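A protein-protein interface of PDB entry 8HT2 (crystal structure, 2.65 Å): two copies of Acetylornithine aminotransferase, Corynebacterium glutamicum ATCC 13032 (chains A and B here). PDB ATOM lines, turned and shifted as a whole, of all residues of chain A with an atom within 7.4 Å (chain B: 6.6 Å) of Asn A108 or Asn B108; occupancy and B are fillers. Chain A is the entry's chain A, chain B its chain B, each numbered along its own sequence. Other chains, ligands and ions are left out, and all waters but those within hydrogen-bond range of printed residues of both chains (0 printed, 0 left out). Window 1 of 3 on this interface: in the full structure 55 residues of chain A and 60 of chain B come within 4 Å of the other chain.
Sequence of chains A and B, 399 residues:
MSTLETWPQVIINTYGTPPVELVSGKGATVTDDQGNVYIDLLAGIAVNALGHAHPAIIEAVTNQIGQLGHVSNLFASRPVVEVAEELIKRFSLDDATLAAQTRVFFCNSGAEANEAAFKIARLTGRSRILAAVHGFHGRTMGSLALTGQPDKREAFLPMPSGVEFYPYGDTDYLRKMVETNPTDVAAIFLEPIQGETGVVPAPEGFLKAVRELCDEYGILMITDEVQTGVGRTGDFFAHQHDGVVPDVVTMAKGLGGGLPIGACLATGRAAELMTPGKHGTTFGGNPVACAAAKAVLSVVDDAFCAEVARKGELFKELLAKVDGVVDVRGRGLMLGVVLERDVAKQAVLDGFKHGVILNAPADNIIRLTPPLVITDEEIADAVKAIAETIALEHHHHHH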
ATOM      1  N   HIS A  70     -10.468   0.543  -6.939  1.00  0.00           N
ATOM      2  CA  HIS A  70      -9.880   1.391  -5.878  1.00  0.00           C
ATOM      3  C   HIS A  70      -8.628   0.717  -5.332  1.00  0.00           C
ATOM      4  O   HIS A  70      -8.582  -0.515  -5.271  1.00  0.00           O
ATOM      5  CB  HIS A  70     -10.892   1.700  -4.779  1.00  0.00           C
ATOM      6  CG  HIS A  70     -10.306   2.376  -3.585  1.00  0.00           C
ATOM      7  ND1 HIS A  70     -10.022   3.725  -3.567  1.00  0.00           N
ATOM      8  CD2 HIS A  70      -9.956   1.899  -2.372  1.00  0.00           C
ATOM      9  CE1 HIS A  70      -9.523   4.050  -2.393  1.00  0.00           C
ATOM     10  NE2 HIS A  70      -9.474   2.947  -1.643  1.00  0.00           N
ATOM     11  N   PHE A 105      -2.233  16.109  -1.668  1.00  0.00           N
ATOM     12  CA  PHE A 105      -3.080  15.092  -0.985  1.00  0.00           C
ATOM     13  C   PHE A 105      -4.415  14.998  -1.735  1.00  0.00           C
ATOM     14  O   PHE A 105      -5.042  16.054  -1.957  1.00  0.00           O
ATOM     15  CB  PHE A 105      -3.271  15.473   0.485  1.00  0.00           C
ATOM     16  CG  PHE A 105      -4.380  14.761   1.224  1.00  0.00           C
ATOM     17  CD1 PHE A 105      -4.151  13.550   1.864  1.00  0.00           C
ATOM     18  CD2 PHE A 105      -5.646  15.328   1.323  1.00  0.00           C
ATOM     19  CE1 PHE A 105      -5.160  12.922   2.580  1.00  0.00           C
ATOM     20  CE2 PHE A 105      -6.657  14.698   2.037  1.00  0.00           C
ATOM     21  CZ  PHE A 105      -6.411  13.499   2.671  1.00  0.00           C
ATOM     22  N   PHE A 106      -4.826  13.786  -2.124  1.00  0.00           N
ATOM     23  CA  PHE A 106      -6.056  13.544  -2.922  1.00  0.00           C
ATOM     24  C   PHE A 106      -7.244  13.237  -2.007  1.00  0.00           C
ATOM     25  O   PHE A 106      -7.082  12.581  -0.976  1.00  0.00           O
ATOM     26  CB  PHE A 106      -5.787  12.469  -3.974  1.00  0.00           C
ATOM     27  CG  PHE A 106      -4.918  13.000  -5.082  1.00  0.00           C
ATOM     28  CD1 PHE A 106      -5.466  13.779  -6.090  1.00  0.00           C
ATOM     29  CD2 PHE A 106      -3.545  12.797  -5.063  1.00  0.00           C
ATOM     30  CE1 PHE A 106      -4.662  14.316  -7.081  1.00  0.00           C
ATOM     31  CE2 PHE A 106      -2.742  13.333  -6.055  1.00  0.00           C
ATOM     32  CZ  PHE A 106      -3.303  14.091  -7.062  1.00  0.00           C
ATOM     33  N   CYS A 107      -8.415  13.749  -2.373  1.00  0.00           N
ATOM     34  CA  CYS A 107      -9.697  13.501  -1.667  1.00  0.00           C
ATOM     35  C   CYS A 107     -10.832  13.498  -2.702  1.00  0.00           C
ATOM     36  O   CYS A 107     -10.518  13.434  -3.910  1.00  0.00           O
ATOM     37  CB  CYS A 107      -9.854  14.524  -0.552  1.00  0.00           C
ATOM     38  SG  CYS A 107      -9.277  16.170  -1.032  1.00  0.00           S
ATOM     39  N   ASN A 108     -12.095  13.566  -2.262  1.00  0.00           N
ATOM     40  CA  ASN A 108     -13.284  13.221  -3.092  1.00  0.00           C
ATOM     41  C   ASN A 108     -14.141  14.458  -3.380  1.00  0.00           C
ATOM     42  O   ASN A 108     -15.099  14.330  -4.149  1.00  0.00           O
ATOM     43  CB  ASN A 108     -14.126  12.125  -2.430  1.00  0.00           C
ATOM     44  CG  ASN A 108     -13.304  10.934  -1.982  1.00  0.00           C
ATOM     45  OD1 ASN A 108     -12.814  10.153  -2.797  1.00  0.00           O
ATOM     46  ND2 ASN A 108     -13.146  10.784  -0.678  1.00  0.00           N
ATOM     47  N   SER A 109     -13.804  15.573  -2.750  1.00  0.00           N
ATOM     48  CA  SER A 109     -14.630  16.798  -2.836  1.00  0.00           C
ATOM     49  C   SER A 109     -13.749  18.006  -2.540  1.00  0.00           C
ATOM     50  O   SER A 109     -12.634  17.816  -2.047  1.00  0.00           O
ATOM     51  CB  SER A 109     -15.815  16.716  -1.911  1.00  0.00           C
ATOM     52  OG  SER A 109     -15.424  16.643  -0.555  1.00  0.00           O
ATOM     53  N   GLY A 110     -14.251  19.194  -2.849  1.00  0.00           N
ATOM     54  CA  GLY A 110     -13.586  20.445  -2.469  1.00  0.00           C
ATOM     55  C   GLY A 110     -13.795  20.758  -1.011  1.00  0.00           C
ATOM     56  O   GLY A 110     -12.868  21.271  -0.389  1.00  0.00           O
ATOM     57  N   ALA A 111     -14.977  20.448  -0.487  1.00  0.00           N
ATOM     58  CA  ALA A 111     -15.163  20.555   0.974  1.00  0.00           C
ATOM     59  C   ALA A 111     -14.093  19.744   1.705  1.00  0.00           C
ATOM     60  O   ALA A 111     -13.526  20.256   2.679  1.00  0.00           O
ATOM     61  CB  ALA A 111     -16.540  20.063   1.298  1.00  0.00           C
ATOM     62  N   GLU A 112     -13.823  18.536   1.227  1.00  0.00           N
ATOM     63  CA  GLU A 112     -12.796  17.662   1.843  1.00  0.00           C
ATOM     64  C   GLU A 112     -11.406  18.267   1.636  1.00  0.00           C
ATOM     65  O   GLU A 112     -10.569  18.119   2.528  1.00  0.00           O
ATOM     66  CB  GLU A 112     -12.892  16.276   1.217  1.00  0.00           C
ATOM     67  CG  GLU A 112     -13.683  15.283   2.041  1.00  0.00           C
ATOM     68  CD  GLU A 112     -13.390  13.847   1.657  1.00  0.00           C
ATOM     69  OE1 GLU A 112     -13.249  13.592   0.458  1.00  0.00           O
ATOM     70  OE2 GLU A 112     -13.289  12.997   2.557  1.00  0.00           O
ATOM     71  N   ALA A 113     -11.187  18.936   0.508  1.00  0.00           N
ATOM     72  CA  ALA A 113      -9.885  19.567   0.210  1.00  0.00           C
ATOM     73  C   ALA A 113      -9.661  20.767   1.127  1.00  0.00           C
ATOM     74  O   ALA A 113      -8.532  20.954   1.595  1.00  0.00           O
ATOM     75  CB  ALA A 113      -9.869  19.975  -1.234  1.00  0.00           C
ATOM     76  N   ALA A 252     -10.699  21.157  -7.028  1.00  0.00           N
ATOM     77  CA  ALA A 252     -11.565  19.967  -7.167  1.00  0.00           C
ATOM     78  C   ALA A 252     -12.337  20.051  -8.477  1.00  0.00           C
ATOM     79  O   ALA A 252     -11.720  19.846  -9.517  1.00  0.00           O
ATOM     80  CB  ALA A 252     -12.534  19.910  -6.023  1.00  0.00           C
ATOM     81  N   LEU A 259     -16.155  13.282 -12.790  1.00  0.00           N
ATOM     82  CA  LEU A 259     -15.929  12.267 -11.744  1.00  0.00           C
ATOM     83  C   LEU A 259     -15.565  12.969 -10.427  1.00  0.00           C
ATOM     84  O   LEU A 259     -14.947  14.037 -10.513  1.00  0.00           O
ATOM     85  CB  LEU A 259     -14.862  11.271 -12.199  1.00  0.00           C
ATOM     86  CG  LEU A 259     -15.403   9.903 -12.602  1.00  0.00           C
ATOM     87  CD1 LEU A 259     -16.258  10.017 -13.846  1.00  0.00           C
ATOM     88  CD2 LEU A 259     -14.283   8.908 -12.828  1.00  0.00           C
ATOM     89  N   PRO A 260     -15.936  12.477  -9.214  1.00  0.00           N
ATOM     90  CA  PRO A 260     -15.633  13.228  -7.998  1.00  0.00           C
ATOM     91  C   PRO A 260     -14.171  13.073  -7.542  1.00  0.00           C
ATOM     92  O   PRO A 260     -13.633  11.972  -7.532  1.00  0.00           O
ATOM     93  CB  PRO A 260     -16.618  12.633  -6.974  1.00  0.00           C
ATOM     94  CG  PRO A 260     -16.820  11.192  -7.436  1.00  0.00           C
ATOM     95  CD  PRO A 260     -16.667  11.224  -8.946  1.00  0.00           C
ATOM     96  N   ILE A 261     -13.573  14.216  -7.198  1.00  0.00           N
ATOM     97  CA  ILE A 261     -12.132  14.397  -6.861  1.00  0.00           C
ATOM     98  C   ILE A 261     -12.000  15.682  -6.041  1.00  0.00           C
ATOM     99  O   ILE A 261     -12.847  16.570  -6.188  1.00  0.00           O
ATOM    100  CB  ILE A 261     -11.265  14.442  -8.133  1.00  0.00           C
ATOM    101  CG1 ILE A 261      -9.809  14.059  -7.854  1.00  0.00           C
ATOM    102  CG2 ILE A 261     -11.375  15.790  -8.825  1.00  0.00           C
ATOM    103  CD1 ILE A 261      -8.970  13.919  -9.097  1.00  0.00           C
ATOM    104  N   GLY A 262     -11.001  15.727  -5.164  1.00  0.00           N
ATOM    105  CA  GLY A 262     -10.401  16.971  -4.668  1.00  0.00           C
ATOM    106  C   GLY A 262      -8.903  16.821  -4.513  1.00  0.00           C
ATOM    107  O   GLY A 262      -8.415  15.690  -4.588  1.00  0.00           O
ATOM    108  N   ALA A 263      -8.208  17.932  -4.290  1.00  0.00           N
ATOM    109  CA  ALA A 263      -6.752  17.939  -4.037  1.00  0.00           C
ATOM    110  C   ALA A 263      -6.374  19.172  -3.204  1.00  0.00           C
ATOM    111  O   ALA A 263      -7.102  20.184  -3.243  1.00  0.00           O
ATOM    112  CB  ALA A 263      -6.018  17.871  -5.348  1.00  0.00           C
ATOM    113  N   GLY A 285     -11.639   4.440  -6.947  1.00  0.00           N
ATOM    114  CA  GLY A 285     -12.137   5.805  -6.732  1.00  0.00           C
ATOM    115  C   GLY A 285     -11.074   6.770  -7.144  1.00  0.00           C
ATOM    116  O   GLY A 285     -11.223   7.359  -8.210  1.00  0.00           O
ATOM    117  N   ASN A 286     -10.032   6.888  -6.327  1.00  0.00           N
ATOM    118  CA  ASN A 286      -8.869   7.723  -6.700  1.00  0.00           C
ATOM    119  C   ASN A 286      -8.355   7.274  -8.068  1.00  0.00           C
ATOM    120  O   ASN A 286      -8.356   8.103  -8.954  1.00  0.00           O
ATOM    121  CB  ASN A 286      -7.812   7.784  -5.591  1.00  0.00           C
ATOM    122  CG  ASN A 286      -8.038   8.926  -4.624  1.00  0.00           C
ATOM    123  OD1 ASN A 286      -8.005  10.091  -5.011  1.00  0.00           O
ATOM    124  ND2 ASN A 286      -8.279   8.600  -3.365  1.00  0.00           N
ATOM    125  N   ALA A 289     -10.857   8.327 -10.798  1.00  0.00           N
ATOM    126  CA  ALA A 289     -11.012   9.791 -10.864  1.00  0.00           C
ATOM    127  C   ALA A 289      -9.690  10.434 -11.274  1.00  0.00           C
ATOM    128  O   ALA A 289      -9.743  11.487 -11.895  1.00  0.00           O
ATOM    129  CB  ALA A 289     -11.491  10.307  -9.542  1.00  0.00           C
ATOM    130  N   PHE B 106     -26.761  11.841  -0.783  1.00  0.00           N
ATOM    131  CA  PHE B 106     -25.530  11.265  -1.368  1.00  0.00           C
ATOM    132  C   PHE B 106     -24.367  12.233  -1.170  1.00  0.00           C
ATOM    133  O   PHE B 106     -24.545  13.437  -1.305  1.00  0.00           O
ATOM    134  CB  PHE B 106     -25.752  10.861  -2.823  1.00  0.00           C
ATOM    135  CG  PHE B 106     -26.596   9.633  -3.031  1.00  0.00           C
ATOM    136  CD1 PHE B 106     -26.018   8.376  -3.050  1.00  0.00           C
ATOM    137  CD2 PHE B 106     -27.963   9.737  -3.219  1.00  0.00           C
ATOM    138  CE1 PHE B 106     -26.793   7.246  -3.245  1.00  0.00           C
ATOM    139  CE2 PHE B 106     -28.736   8.605  -3.413  1.00  0.00           C
ATOM    140  CZ  PHE B 106     -28.150   7.363  -3.426  1.00  0.00           C
ATOM    141  N   CYS B 107     -23.212  11.667  -0.840  1.00  0.00           N
ATOM    142  CA  CYS B 107     -21.931  12.390  -0.660  1.00  0.00           C
ATOM    143  C   CYS B 107     -20.881  11.712  -1.544  1.00  0.00           C
ATOM    144  O   CYS B 107     -21.271  11.093  -2.534  1.00  0.00           O
ATOM    145  CB  CYS B 107     -21.492  12.323   0.797  1.00  0.00           C
ATOM    146  SG  CYS B 107     -22.710  11.565   1.893  1.00  0.00           S
ATOM    147  N   ASN B 108     -19.606  11.805  -1.172  1.00  0.00           N
ATOM    148  CA  ASN B 108     -18.499  11.264  -2.002  1.00  0.00           C
ATOM    149  C   ASN B 108     -17.567  10.418  -1.134  1.00  0.00           C
ATOM    150  O   ASN B 108     -16.739   9.699  -1.695  1.00  0.00           O
ATOM    151  CB  ASN B 108     -17.764  12.363  -2.773  1.00  0.00           C
ATOM    152  CG  ASN B 108     -18.675  13.206  -3.630  1.00  0.00           C
ATOM    153  OD1 ASN B 108     -19.295  12.703  -4.560  1.00  0.00           O
ATOM    154  ND2 ASN B 108     -18.758  14.488  -3.325  1.00  0.00           N
ATOM    155  N   SER B 109     -17.724  10.491   0.183  1.00  0.00           N
ATOM    156  CA  SER B 109     -16.955   9.629   1.111  1.00  0.00           C
ATOM    157  C   SER B 109     -17.829   9.234   2.301  1.00  0.00           C
ATOM    158  O   SER B 109     -18.975   9.672   2.359  1.00  0.00           O
ATOM    159  CB  SER B 109     -15.682  10.285   1.557  1.00  0.00           C
ATOM    160  OG  SER B 109     -15.930  11.537   2.168  1.00  0.00           O
ATOM    161  N   GLY B 110     -17.277   8.437   3.211  1.00  0.00           N
ATOM    162  CA  GLY B 110     -17.937   8.103   4.482  1.00  0.00           C
ATOM    163  C   GLY B 110     -17.694   9.163   5.524  1.00  0.00           C
ATOM    164  O   GLY B 110     -18.543   9.361   6.383  1.00  0.00           O
ATOM    165  N   GLU B 112     -17.621  12.326   4.572  1.00  0.00           N
ATOM    166  CA  GLU B 112     -18.611  13.326   4.104  1.00  0.00           C
ATOM    167  C   GLU B 112     -20.015  12.862   4.505  1.00  0.00           C
ATOM    168  O   GLU B 112     -20.904  13.704   4.668  1.00  0.00           O
ATOM    169  CB  GLU B 112     -18.436  13.526   2.602  1.00  0.00           C
ATOM    170  CG  GLU B 112     -18.639  14.956   2.150  1.00  0.00           C
ATOM    171  CD  GLU B 112     -18.557  15.141   0.647  1.00  0.00           C
ATOM    172  OE1 GLU B 112     -18.434  14.130  -0.055  1.00  0.00           O
ATOM    173  OE2 GLU B 112     -18.620  16.294   0.187  1.00  0.00           O
ATOM    174  N   ALA B 113     -20.171  11.556   4.692  1.00  0.00           N
ATOM    175  CA  ALA B 113     -21.463  10.936   5.037  1.00  0.00           C
ATOM    176  C   ALA B 113     -21.740  11.160   6.510  1.00  0.00           C
ATOM    177  O   ALA B 113     -22.851  11.571   6.850  1.00  0.00           O
ATOM    178  CB  ALA B 113     -21.402   9.470   4.750  1.00  0.00           C
ATOM    179  N   ALA B 252     -20.755   4.044   2.531  1.00  0.00           N
ATOM    180  CA  ALA B 252     -19.757   4.479   1.531  1.00  0.00           C
ATOM    181  C   ALA B 252     -19.077   3.246   0.927  1.00  0.00           C
ATOM    182  O   ALA B 252     -19.756   2.477   0.230  1.00  0.00           O
ATOM    183  CB  ALA B 252     -18.774   5.428   2.169  1.00  0.00           C
ATOM    184  N   LEU B 259     -15.533   3.204  -6.637  1.00  0.00           N
ATOM    185  CA  LEU B 259     -15.704   4.608  -7.095  1.00  0.00           C
ATOM    186  C   LEU B 259     -16.020   5.472  -5.870  1.00  0.00           C
ATOM    187  O   LEU B 259     -16.485   4.902  -4.872  1.00  0.00           O
ATOM    188  CB  LEU B 259     -16.820   4.680  -8.143  1.00  0.00           C
ATOM    189  CG  LEU B 259     -16.381   4.531  -9.598  1.00  0.00           C
ATOM    190  CD1 LEU B 259     -17.402   5.142 -10.536  1.00  0.00           C
ATOM    191  CD2 LEU B 259     -15.030   5.176  -9.824  1.00  0.00           C
ATOM    192  N   PRO B 260     -15.764   6.800  -5.881  1.00  0.00           N
ATOM    193  CA  PRO B 260     -16.018   7.642  -4.721  1.00  0.00           C
ATOM    194  C   PRO B 260     -17.514   7.876  -4.468  1.00  0.00           C
ATOM    195  O   PRO B 260     -18.166   8.386  -5.344  1.00  0.00           O
ATOM    196  CB  PRO B 260     -15.288   8.951  -5.033  1.00  0.00           C
ATOM    197  CG  PRO B 260     -14.416   8.630  -6.219  1.00  0.00           C
ATOM    198  CD  PRO B 260     -15.195   7.580  -6.977  1.00  0.00           C
ATOM    199  N   ILE B 261     -18.015   7.420  -3.321  1.00  0.00           N
ATOM    200  CA  ILE B 261     -19.449   7.547  -2.934  1.00  0.00           C
ATOM    201  C   ILE B 261     -19.551   7.505  -1.412  1.00  0.00           C
ATOM    202  O   ILE B 261     -18.671   6.928  -0.767  1.00  0.00           O
ATOM    203  CB  ILE B 261     -20.327   6.457  -3.581  1.00  0.00           C
ATOM    204  CG1 ILE B 261     -21.748   6.955  -3.842  1.00  0.00           C
ATOM    205  CG2 ILE B 261     -20.317   5.177  -2.762  1.00  0.00           C
ATOM    206  CD1 ILE B 261     -22.593   5.991  -4.630  1.00  0.00           C
ATOM    207  N   GLY B 262     -20.584   8.159  -0.897  1.00  0.00           N
ATOM    208  CA  GLY B 262     -21.155   7.929   0.435  1.00  0.00           C
ATOM    209  C   GLY B 262     -22.649   8.170   0.423  1.00  0.00           C
ATOM    210  O   GLY B 262     -23.145   8.694  -0.576  1.00  0.00           O
ATOM    211  N   ALA B 263     -23.330   7.808   1.506  1.00  0.00           N
ATOM    212  CA  ALA B 263     -24.764   8.123   1.633  1.00  0.00           C
ATOM    213  C   ALA B 263     -25.204   8.211   3.101  1.00  0.00           C
ATOM    214  O   ALA B 263     -24.741   7.410   3.917  1.00  0.00           O
ATOM    215  CB  ALA B 263     -25.571   7.135   0.844  1.00  0.00           C
ATOM    216  N   THR B 281     -23.997  18.580  -1.130  1.00  0.00           N
ATOM    217  CA  THR B 281     -22.630  18.529  -1.712  1.00  0.00           C
ATOM    218  C   THR B 281     -22.715  18.757  -3.220  1.00  0.00           C
ATOM    219  O   THR B 281     -23.774  18.474  -3.790  1.00  0.00           O
ATOM    220  CB  THR B 281     -21.864  17.253  -1.347  1.00  0.00           C
ATOM    221  OG1 THR B 281     -20.784  17.073  -2.264  1.00  0.00           O
ATOM    222  CG2 THR B 281     -22.728  16.020  -1.355  1.00  0.00           C
ATOM    223  N   THR B 282     -21.639  19.267  -3.824  1.00  0.00           N
ATOM    224  CA  THR B 282     -21.619  19.465  -5.291  1.00  0.00           C
ATOM    225  C   THR B 282     -21.857  18.127  -5.995  1.00  0.00           C
ATOM    226  O   THR B 282     -22.887  18.016  -6.680  1.00  0.00           O
ATOM    227  CB  THR B 282     -20.309  20.114  -5.743  1.00  0.00           C
ATOM    228  OG1 THR B 282     -20.139  21.307  -4.977  1.00  0.00           O
ATOM    229  CG2 THR B 282     -20.328  20.442  -7.219  1.00  0.00           C
ATOM    230  N   PHE B 283     -20.956  17.151  -5.808  1.00  0.00           N
ATOM    231  CA  PHE B 283     -21.077  15.834  -6.493  1.00  0.00           C
ATOM    232  C   PHE B 283     -22.092  14.932  -5.783  1.00  0.00           C
ATOM    233  O   PHE B 283     -22.015  13.713  -5.940  1.00  0.00           O
ATOM    234  CB  PHE B 283     -19.719  15.157  -6.693  1.00  0.00           C
ATOM    235  CG  PHE B 283     -18.536  16.049  -6.957  1.00  0.00           C
ATOM    236  CD1 PHE B 283     -18.403  16.721  -8.159  1.00  0.00           C
ATOM    237  CD2 PHE B 283     -17.524  16.170  -6.021  1.00  0.00           C
ATOM    238  CE1 PHE B 283     -17.300  17.522  -8.400  1.00  0.00           C
ATOM    239  CE2 PHE B 283     -16.419  16.968  -6.266  1.00  0.00           C
ATOM    240  CZ  PHE B 283     -16.309  17.642  -7.455  1.00  0.00           C
ATOM    241  N   GLY B 284     -23.005  15.511  -5.010  1.00  0.00           N
ATOM    242  CA  GLY B 284     -24.081  14.713  -4.399  1.00  0.00           C
ATOM    243  C   GLY B 284     -24.962  14.166  -5.489  1.00  0.00           C
ATOM    244  O   GLY B 284     -25.500  14.970  -6.262  1.00  0.00           O
ATOM    245  N   GLY B 285     -25.079  12.847  -5.575  1.00  0.00           N
ATOM    246  CA  GLY B 285     -25.810  12.269  -6.708  1.00  0.00           C
ATOM    247  C   GLY B 285     -24.937  12.264  -7.941  1.00  0.00           C
ATOM    248  O   GLY B 285     -25.439  12.676  -8.988  1.00  0.00           O
ATOM    249  N   ASN B 286     -23.678  11.831  -7.811  1.00  0.00           N
ATOM    250  CA  ASN B 286     -22.770  11.730  -8.981  1.00  0.00           C
ATOM    251  C   ASN B 286     -23.260  10.617  -9.918  1.00  0.00           C
ATOM    252  O   ASN B 286     -23.216   9.468  -9.485  1.00  0.00           O
ATOM    253  CB  ASN B 286     -21.286  11.594  -8.638  1.00  0.00           C
ATOM    254  CG  ASN B 286     -20.382  11.827  -9.829  1.00  0.00           C
ATOM    255  OD1 ASN B 286     -20.047  10.897 -10.554  1.00  0.00           O
ATOM    256  ND2 ASN B 286     -19.984  13.069 -10.034  1.00  0.00           N
ATOM    257  N   ALA B 289     -20.517   7.603 -10.349  1.00  0.00           N
ATOM    258  CA  ALA B 289     -20.449   7.070  -8.966  1.00  0.00           C
ATOM    259  C   ALA B 289     -21.681   6.207  -8.652  1.00  0.00           C
ATOM    260  O   ALA B 289     -21.492   5.172  -7.982  1.00  0.00           O
ATOM    261  CB  ALA B 289     -20.323   8.200  -7.971  1.00  0.00           C
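OG of Ser A109 is in hydrogen-bond range of OE2 of Glu B112.
OG of Ser B109 is in hydrogen-bond range of OE2 of Glu A112, 3.0 Å away.
O of Asn A108 lies within hydrogen-bond range of N of Ile A261 (3.4 Å).
The backbone NH of Asn B108 is in hydrogen-bond range of the side-chain carboxylate of Glu B112.
The side-chain amide oxygen (OD1) of Asn B108 lies close to the backbone carbonyl oxygen (O) of Phe B283 (3.2 Å).
The side-chain hydroxyl (OG) of Ser B109 lies within hydrogen-bond range of the backbone NH (N) of Glu B112, at 3.0 Å.
The side-chain hydroxyl of Thr B281 lies within hydrogen-bond range of the side-chain carboxylate of Glu B112.
The side-chain amide oxygen (OD1) of Asn B286 sits at hydrogen-bond distance from the backbone NH (N) of Ala B289 (3.3 Å).
Among the printed residues, pairs that only touch across the chains: Asn A108 with Asn B108 (3.6 Å), Asn A108 with Ser B109 (3.4 Å), Asn A108 with Pro B260 (3.5 Å), Asn A108 with Phe B283 (3.6 Å), Ser A109 with Asn B108 (3.95 Å), Ser A109 with Phe B283 (3.9 Å), Pro A260 with Asn B108 (3.6 Å), Pro A260 with Pro B260 (3.6 Å), Pro A260 with Phe B283 (3.8 Å), Pro A260 with Asn B286 (3.8 Å), Ile A261 with Phe B283 (3.6 Å), Gly A285 with Leu B259 (3.8 Å) and Gly A285 with Pro B260 (3.5 Å).
Of chain B, only Asn B108, Ser B109, Pro B260 and Phe B283 come within 4 Å of Asn A108.
Asn B108 touches just these residues of chain A: Asn A108 (3.6 Å), Ser A109 (3.95 Å) and Pro A260 (3.6 Å).
Printed residues of chain A within 4 Å of Ser B109: Asn A108 (3.4 Å) and Glu A112 (3.0 Å).
Of the printed residues of chain A, Asn B286 touches Pro A260.
Of the printed residues of chain B, Gly A285 touches Leu B259 (3.8 Å) and Pro B260 (3.5 Å).
The nearest residue of chain A that does not touch Asn B108 is Glu A112 (5.6 Å).
Along chain A the printed residues that touch a printed residue of chain B span positions 108 to 285.
Printed residues of chain B that touch a printed residue of chain A: Asn B108, Ser B109, Glu B112, Leu B259, Pro B260, Phe B283 and Asn B286.
Asn B108 touches its own counterpart, Asn A108.
Asn A108 touches Pro B260, and with the chains exchanged Pro A260 touches Asn B108.
Ser A109 touches Glu B112, and with the chains exchanged Glu A112 touches Ser B109.
Pro A260 touches its own counterpart, Pro B260.
Positions printed for both chains: 106, 107, 108, 109, 110, 112, 113, 252, 259, 260, 261, 262, 263, 285, 286 and 289.
Of the 15 pairs that touch across the chains among the printed residues, 8 have their exchanged pair printed and touching as well.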
